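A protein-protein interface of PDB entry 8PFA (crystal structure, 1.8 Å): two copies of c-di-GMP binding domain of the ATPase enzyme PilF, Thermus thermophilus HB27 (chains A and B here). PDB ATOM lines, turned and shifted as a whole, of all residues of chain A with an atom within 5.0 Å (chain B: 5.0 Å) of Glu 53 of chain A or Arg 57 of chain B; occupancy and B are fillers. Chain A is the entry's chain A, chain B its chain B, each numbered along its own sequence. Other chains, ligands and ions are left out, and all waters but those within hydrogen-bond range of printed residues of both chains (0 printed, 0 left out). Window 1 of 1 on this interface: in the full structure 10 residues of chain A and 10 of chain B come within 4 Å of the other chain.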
ATOM      1  N   PRO A  51      -9.425  -8.742 -26.105  1.00  0.00           N
ATOM      2  CA  PRO A  51      -8.066  -9.254 -25.907  1.00  0.00           C
ATOM      3  C   PRO A  51      -7.891 -10.571 -26.642  1.00  0.00           C
ATOM      4  O   PRO A  51      -8.767 -11.437 -26.628  1.00  0.00           O
ATOM      5  CB  PRO A  51      -7.956  -9.434 -24.389  1.00  0.00           C
ATOM      6  CG  PRO A  51      -8.904  -8.381 -23.824  1.00  0.00           C
ATOM      7  CD  PRO A  51     -10.078  -8.437 -24.822  1.00  0.00           C
ATOM      8  N   GLU A  52      -6.754 -10.707 -27.315  1.00  0.00           N
ATOM      9  CA  GLU A  52      -6.523 -11.955 -28.050  1.00  0.00           C
ATOM     10  C   GLU A  52      -6.594 -13.174 -27.127  1.00  0.00           C
ATOM     11  O   GLU A  52      -7.087 -14.234 -27.532  1.00  0.00           O
ATOM     12  CB  GLU A  52      -5.177 -11.875 -28.776  1.00  0.00           C
ATOM     13  CG  GLU A  52      -4.688 -13.170 -29.406  1.00  0.00           C
ATOM     14  CD  GLU A  52      -3.262 -13.045 -29.950  1.00  0.00           C
ATOM     15  OE1 GLU A  52      -2.331 -12.777 -29.158  1.00  0.00           O
ATOM     16  OE2 GLU A  52      -3.079 -13.200 -31.176  1.00  0.00           O
ATOM     17  N   GLU A  53      -6.147 -13.044 -25.871  1.00  0.00           N
ATOM     18  CA  GLU A  53      -6.248 -14.195 -24.969  1.00  0.00           C
ATOM     19  C   GLU A  53      -7.695 -14.530 -24.625  1.00  0.00           C
ATOM     20  O   GLU A  53      -8.020 -15.702 -24.401  1.00  0.00           O
ATOM     21  CB  GLU A  53      -5.462 -13.963 -23.678  1.00  0.00           C
ATOM     22  CG  GLU A  53      -5.296 -15.239 -22.884  1.00  0.00           C
ATOM     23  CD  GLU A  53      -4.554 -15.054 -21.571  1.00  0.00           C
ATOM     24  OE1 GLU A  53      -5.206 -14.699 -20.566  1.00  0.00           O
ATOM     25  OE2 GLU A  53      -3.322 -15.277 -21.559  1.00  0.00           O
ATOM     26  N   ALA A  54      -8.570 -13.526 -24.556  1.00  0.00           N
ATOM     27  CA  ALA A  54      -9.988 -13.805 -24.349  1.00  0.00           C
ATOM     28  C   ALA A  54     -10.548 -14.641 -25.497  1.00  0.00           C
ATOM     29  O   ALA A  54     -11.288 -15.612 -25.281  1.00  0.00           O
ATOM     30  CB  ALA A  54     -10.749 -12.480 -24.194  1.00  0.00           C
ATOM     31  N   LEU A  55     -10.189 -14.281 -26.729  1.00  0.00           N
ATOM     32  CA  LEU A  55     -10.607 -15.057 -27.883  1.00  0.00           C
ATOM     33  C   LEU A  55     -10.124 -16.495 -27.767  1.00  0.00           C
ATOM     34  O   LEU A  55     -10.886 -17.441 -27.991  1.00  0.00           O
ATOM     35  CB  LEU A  55     -10.078 -14.405 -29.163  1.00  0.00           C
ATOM     36  CG  LEU A  55     -10.255 -15.256 -30.426  1.00  0.00           C
ATOM     37  CD1 LEU A  55     -11.752 -15.435 -30.742  1.00  0.00           C
ATOM     38  CD2 LEU A  55      -9.524 -14.611 -31.606  1.00  0.00           C
ATOM     39  N   TYR A  56      -8.860 -16.686 -27.397  1.00  0.00           N
ATOM     40  CA  TYR A  56      -8.341 -18.051 -27.422  1.00  0.00           C
ATOM     41  C   TYR A  56      -8.912 -18.879 -26.285  1.00  0.00           C
ATOM     42  O   TYR A  56      -9.181 -20.070 -26.469  1.00  0.00           O
ATOM     43  CB  TYR A  56      -6.821 -18.048 -27.392  1.00  0.00           C
ATOM     44  CG  TYR A  56      -6.260 -17.992 -28.788  1.00  0.00           C
ATOM     45  CD1 TYR A  56      -6.344 -16.821 -29.536  1.00  0.00           C
ATOM     46  CD2 TYR A  56      -5.647 -19.100 -29.361  1.00  0.00           C
ATOM     47  CE1 TYR A  56      -5.845 -16.758 -30.822  1.00  0.00           C
ATOM     48  CE2 TYR A  56      -5.137 -19.044 -30.659  1.00  0.00           C
ATOM     49  CZ  TYR A  56      -5.247 -17.871 -31.381  1.00  0.00           C
ATOM     50  OH  TYR A  56      -4.758 -17.791 -32.665  1.00  0.00           O
ATOM     51  N   ARG A  57      -9.130 -18.272 -25.118  1.00  0.00           N
ATOM     52  CA  ARG A  57      -9.765 -19.012 -24.023  1.00  0.00           C
ATOM     53  C   ARG A  57     -11.162 -19.493 -24.422  1.00  0.00           C
ATOM     54  O   ARG A  57     -11.552 -20.624 -24.102  1.00  0.00           O
ATOM     55  CB  ARG A  57      -9.828 -18.151 -22.758  1.00  0.00           C
ATOM     56  CG  ARG A  57      -8.448 -17.986 -22.062  1.00  0.00           C
ATOM     57  CD  ARG A  57      -8.567 -17.045 -20.867  1.00  0.00           C
ATOM     58  NE  ARG A  57      -7.260 -16.728 -20.247  1.00  0.00           N
ATOM     59  CZ  ARG A  57      -6.615 -17.537 -19.411  1.00  0.00           C
ATOM     60  NH1 ARG A  57      -5.443 -17.175 -18.881  1.00  0.00           N
ATOM     61  NH2 ARG A  57      -7.136 -18.718 -19.121  1.00  0.00           N
ATOM     62  N   ALA A  58     -11.916 -18.657 -25.143  1.00  0.00           N
ATOM     63  CA  ALA A  58     -13.255 -19.048 -25.594  1.00  0.00           C
ATOM     64  C   ALA A  58     -13.189 -20.129 -26.670  1.00  0.00           C
ATOM     65  O   ALA A  58     -13.967 -21.090 -26.647  1.00  0.00           O
ATOM     66  CB  ALA A  58     -13.995 -17.833 -26.134  1.00  0.00           C
ATOM     67  N   PHE A  67      -6.529 -24.567 -22.552  1.00  0.00           N
ATOM     68  CA  PHE A  67      -5.754 -23.409 -22.958  1.00  0.00           C
ATOM     69  C   PHE A  67      -4.465 -23.364 -22.149  1.00  0.00           C
ATOM     70  O   PHE A  67      -4.492 -23.510 -20.924  1.00  0.00           O
ATOM     71  CB  PHE A  67      -6.550 -22.120 -22.735  1.00  0.00           C
ATOM     72  CG  PHE A  67      -5.761 -20.880 -23.008  1.00  0.00           C
ATOM     73  CD1 PHE A  67      -5.366 -20.573 -24.291  1.00  0.00           C
ATOM     74  CD2 PHE A  67      -5.385 -20.023 -21.961  1.00  0.00           C
ATOM     75  CE1 PHE A  67      -4.608 -19.444 -24.554  1.00  0.00           C
ATOM     76  CE2 PHE A  67      -4.650 -18.890 -22.224  1.00  0.00           C
ATOM     77  CZ  PHE A  67      -4.262 -18.597 -23.520  1.00  0.00           C
ATOM     78  N   LEU A 131      -1.381 -19.578 -27.570  1.00  0.00           N
ATOM     79  CA  LEU A 131      -1.326 -18.345 -28.335  1.00  0.00           C
ATOM     80  C   LEU A 131      -0.262 -18.438 -29.427  1.00  0.00           C
ATOM     81  O   LEU A 131       0.701 -19.200 -29.306  1.00  0.00           O
ATOM     82  CB  LEU A 131      -0.996 -17.165 -27.402  1.00  0.00           C
ATOM     83  CG  LEU A 131      -2.065 -16.888 -26.351  1.00  0.00           C
ATOM     84  CD1 LEU A 131      -1.611 -15.868 -25.306  1.00  0.00           C
ATOM     85  CD2 LEU A 131      -3.325 -16.410 -27.059  1.00  0.00           C
ATOM     86  N   TRP B  21     -11.393  -6.572 -20.794  1.00  0.00           N
ATOM     87  CA  TRP B  21     -11.717  -7.753 -20.000  1.00  0.00           C
ATOM     88  C   TRP B  21     -13.028  -7.605 -19.241  1.00  0.00           C
ATOM     89  O   TRP B  21     -13.664  -8.610 -18.900  1.00  0.00           O
ATOM     90  CB  TRP B  21     -10.592  -8.027 -19.016  1.00  0.00           C
ATOM     91  CG  TRP B  21      -9.426  -8.710 -19.656  1.00  0.00           C
ATOM     92  CD1 TRP B  21      -8.202  -8.172 -19.925  1.00  0.00           C
ATOM     93  CD2 TRP B  21      -9.385 -10.066 -20.113  1.00  0.00           C
ATOM     94  NE1 TRP B  21      -7.397  -9.120 -20.526  1.00  0.00           N
ATOM     95  CE2 TRP B  21      -8.105 -10.285 -20.650  1.00  0.00           C
ATOM     96  CE3 TRP B  21     -10.312 -11.113 -20.128  1.00  0.00           C
ATOM     97  CZ2 TRP B  21      -7.720 -11.514 -21.177  1.00  0.00           C
ATOM     98  CZ3 TRP B  21      -9.930 -12.331 -20.657  1.00  0.00           C
ATOM     99  CH2 TRP B  21      -8.644 -12.521 -21.167  1.00  0.00           C
ATOM    100  N   PRO B  51      -9.895 -13.965 -15.916  1.00  0.00           N
ATOM    101  CA  PRO B  51      -8.810 -14.928 -15.661  1.00  0.00           C
ATOM    102  C   PRO B  51      -7.815 -14.370 -14.658  1.00  0.00           C
ATOM    103  O   PRO B  51      -7.419 -13.204 -14.733  1.00  0.00           O
ATOM    104  CB  PRO B  51      -8.173 -15.129 -17.044  1.00  0.00           C
ATOM    105  CG  PRO B  51      -9.332 -14.863 -18.014  1.00  0.00           C
ATOM    106  CD  PRO B  51     -10.097 -13.726 -17.358  1.00  0.00           C
ATOM    107  N   GLU B  53      -4.758 -14.908 -14.533  1.00  0.00           N
ATOM    108  CA  GLU B  53      -3.570 -14.443 -15.256  1.00  0.00           C
ATOM    109  C   GLU B  53      -3.761 -13.046 -15.827  1.00  0.00           C
ATOM    110  O   GLU B  53      -2.813 -12.258 -15.871  1.00  0.00           O
ATOM    111  CB  GLU B  53      -3.205 -15.414 -16.375  1.00  0.00           C
ATOM    112  CG  GLU B  53      -2.813 -16.792 -15.864  1.00  0.00           C
ATOM    113  CD  GLU B  53      -4.005 -17.627 -15.352  1.00  0.00           C
ATOM    114  OE1 GLU B  53      -5.184 -17.252 -15.617  1.00  0.00           O
ATOM    115  OE2 GLU B  53      -3.775 -18.662 -14.695  1.00  0.00           O
ATOM    116  N   ALA B  54      -4.967 -12.729 -16.312  1.00  0.00           N
ATOM    117  CA  ALA B  54      -5.201 -11.372 -16.798  1.00  0.00           C
ATOM    118  C   ALA B  54      -5.112 -10.372 -15.658  1.00  0.00           C
ATOM    119  O   ALA B  54      -4.598  -9.256 -15.830  1.00  0.00           O
ATOM    120  CB  ALA B  54      -6.565 -11.285 -17.501  1.00  0.00           C
ATOM    121  N   LEU B  55      -5.621 -10.747 -14.484  1.00  0.00           N
ATOM    122  CA  LEU B  55      -5.507  -9.867 -13.326  1.00  0.00           C
ATOM    123  C   LEU B  55      -4.045  -9.589 -13.006  1.00  0.00           C
ATOM    124  O   LEU B  55      -3.647  -8.437 -12.795  1.00  0.00           O
ATOM    125  CB  LEU B  55      -6.209 -10.489 -12.113  1.00  0.00           C
ATOM    126  CG  LEU B  55      -5.988  -9.742 -10.785  1.00  0.00           C
ATOM    127  CD1 LEU B  55      -6.556  -8.345 -10.859  1.00  0.00           C
ATOM    128  CD2 LEU B  55      -6.626 -10.499  -9.612  1.00  0.00           C
ATOM    129  N   TYR B  56      -3.226 -10.636 -12.973  1.00  0.00           N
ATOM    130  CA  TYR B  56      -1.850 -10.442 -12.532  1.00  0.00           C
ATOM    131  C   TYR B  56      -1.029  -9.697 -13.572  1.00  0.00           C
ATOM    132  O   TYR B  56      -0.121  -8.943 -13.210  1.00  0.00           O
ATOM    133  CB  TYR B  56      -1.220 -11.784 -12.190  1.00  0.00           C
ATOM    134  CG  TYR B  56      -1.405 -12.137 -10.742  1.00  0.00           C
ATOM    135  CD1 TYR B  56      -2.666 -12.136 -10.169  1.00  0.00           C
ATOM    136  CD2 TYR B  56      -0.312 -12.446  -9.935  1.00  0.00           C
ATOM    137  CE1 TYR B  56      -2.841 -12.450  -8.835  1.00  0.00           C
ATOM    138  CE2 TYR B  56      -0.473 -12.752  -8.600  1.00  0.00           C
ATOM    139  CZ  TYR B  56      -1.737 -12.759  -8.055  1.00  0.00           C
ATOM    140  OH  TYR B  56      -1.910 -13.069  -6.727  1.00  0.00           O
ATOM    141  N   ARG B  57      -1.343  -9.863 -14.860  1.00  0.00           N
ATOM    142  CA  ARG B  57      -0.666  -9.050 -15.868  1.00  0.00           C
ATOM    143  C   ARG B  57      -0.975  -7.568 -15.678  1.00  0.00           C
ATOM    144  O   ARG B  57      -0.085  -6.721 -15.834  1.00  0.00           O
ATOM    145  CB  ARG B  57      -1.053  -9.501 -17.288  1.00  0.00           C
ATOM    146  CG  ARG B  57      -0.333 -10.759 -17.763  1.00  0.00           C
ATOM    147  CD  ARG B  57      -0.494 -11.000 -19.277  1.00  0.00           C
ATOM    148  NE  ARG B  57      -1.896 -11.125 -19.652  1.00  0.00           N
ATOM    149  CZ  ARG B  57      -2.570 -12.274 -19.678  1.00  0.00           C
ATOM    150  NH1 ARG B  57      -3.848 -12.282 -20.036  1.00  0.00           N
ATOM    151  NH2 ARG B  57      -1.975 -13.415 -19.347  1.00  0.00           N
ATOM    152  N   ALA B  58      -2.237  -7.233 -15.357  1.00  0.00           N
ATOM    153  CA  ALA B  58      -2.604  -5.839 -15.123  1.00  0.00           C
ATOM    154  C   ALA B  58      -1.930  -5.293 -13.870  1.00  0.00           C
ATOM    155  O   ALA B  58      -1.443  -4.159 -13.864  1.00  0.00           O
ATOM    156  CB  ALA B  58      -4.123  -5.709 -14.993  1.00  0.00           C
ATOM    157  N   LEU B  59      -1.905  -6.085 -12.797  1.00  0.00           N
ATOM    158  CA  LEU B  59      -1.260  -5.649 -11.558  1.00  0.00           C
ATOM    159  C   LEU B  59       0.242  -5.467 -11.763  1.00  0.00           C
ATOM    160  O   LEU B  59       0.841  -4.525 -11.235  1.00  0.00           O
ATOM    161  CB  LEU B  59      -1.548  -6.671 -10.457  1.00  0.00           C
ATOM    162  CG  LEU B  59      -2.980  -6.697  -9.911  1.00  0.00           C
ATOM    163  CD1 LEU B  59      -3.187  -7.878  -8.988  1.00  0.00           C
ATOM    164  CD2 LEU B  59      -3.316  -5.393  -9.184  1.00  0.00           C
ATOM    165  N   ALA B  60       0.861  -6.339 -12.562  1.00  0.00           N
ATOM    166  CA  ALA B  60       2.276  -6.165 -12.886  1.00  0.00           C
ATOM    167  C   ALA B  60       2.512  -4.889 -13.681  1.00  0.00           C
ATOM    168  O   ALA B  60       3.468  -4.152 -13.415  1.00  0.00           O
ATOM    169  CB  ALA B  60       2.789  -7.380 -13.654  1.00  0.00           C
ATOM    170  N   GLU B  61       1.658  -4.617 -14.674  1.00  0.00           N
ATOM    171  CA  GLU B  61       1.796  -3.386 -15.445  1.00  0.00           C
ATOM    172  C   GLU B  61       1.696  -2.171 -14.538  1.00  0.00           C
ATOM    173  O   GLU B  61       2.407  -1.182 -14.732  1.00  0.00           O
ATOM    174  CB  GLU B  61       0.710  -3.315 -16.517  1.00  0.00           C
ATOM    175  CG  GLU B  61       0.966  -4.136 -17.753  1.00  0.00           C
ATOM    176  CD  GLU B  61       0.012  -3.756 -18.875  1.00  0.00           C
ATOM    177  OE1 GLU B  61      -0.105  -2.546 -19.181  1.00  0.00           O
ATOM    178  OE2 GLU B  61      -0.642  -4.666 -19.422  1.00  0.00           O
ATOM    179  N   PHE B  67       5.557  -9.716 -15.389  1.00  0.00           N
ATOM    180  CA  PHE B  67       4.789 -10.888 -15.005  1.00  0.00           C
ATOM    181  C   PHE B  67       5.417 -12.134 -15.613  1.00  0.00           C
ATOM    182  O   PHE B  67       5.759 -12.148 -16.800  1.00  0.00           O
ATOM    183  CB  PHE B  67       3.328 -10.767 -15.449  1.00  0.00           C
ATOM    184  CG  PHE B  67       2.524 -12.008 -15.183  1.00  0.00           C
ATOM    185  CD1 PHE B  67       2.270 -12.418 -13.883  1.00  0.00           C
ATOM    186  CD2 PHE B  67       2.041 -12.780 -16.229  1.00  0.00           C
ATOM    187  CE1 PHE B  67       1.547 -13.570 -13.622  1.00  0.00           C
ATOM    188  CE2 PHE B  67       1.309 -13.924 -15.978  1.00  0.00           C
ATOM    189  CZ  PHE B  67       1.050 -14.315 -14.676  1.00  0.00           C
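The guanidinium group of Arg 57 of chain B is in salt-bridge range of the side-chain carboxylate of Glu 53 of chain A (2.8 Å). The guanidinium group of Arg 57 of chain A is in salt-bridge range of the side-chain carboxylate of Glu 53 of chain B.
The side-chain carboxylate (OE1) of Glu 53 of chain A is in salt-bridge range of the guanidinium group (NE) of Arg 57 of chain A (2.9 Å).
Trp 21 of chain B touches Pro 51 of chain A (NE1 to CG, 3.7 Å). CH2 of Trp 21 of chain B touches N of Ala 54 of chain A, at 3.5 Å. NE of Arg 57 of chain A touches CG of Pro 51 of chain B (3.6 Å).
Printed residues of chain B within 4 Å of Pro 51 of chain A: Trp 21 (3.7 Å). Of chain B, only Arg 57 (2.8 Å) comes within 4 Å of Glu 53 of chain A. Printed residues of chain B within 4 Å of Ala 54 of chain A: Trp 21. Printed residues of chain A within 4 Å of Trp 21 of chain B: Pro 51 and Ala 54. Printed residues of chain A within 4 Å of Glu 53 of chain B: Arg 57 (3.3 Å). Of chain A, only Glu 53 comes within 4 Å of Arg 57 of chain B. Ala 58 of chain B touches none of the printed residues of chain A. The nearest printed residue of chain A that does not touch Trp 21 of chain B is Glu 53 of chain A (4.1 Å).
Of the 10 printed residues of chain A, 4 touch a printed residue of chain B. Hydrophobic or aromatic side chains of chain A within 4 Å of the printed part of chain B: Pro 51 and Ala 54. Among the printed residues, 5 pairs touch across the chains.
Glu 53 of chain A touches Arg 57 of chain B, and with the chains exchanged Arg 57 of chain A touches Glu 53 of chain B. Arg 57 of chain A touches Pro 51 of chain B, but with the chains exchanged Pro 51 of chain A does not touch Arg 57 of chain B (6.6 Å). Positions printed for both chains: 51, 53, 54, 55, 56, 57, 58 and 67.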
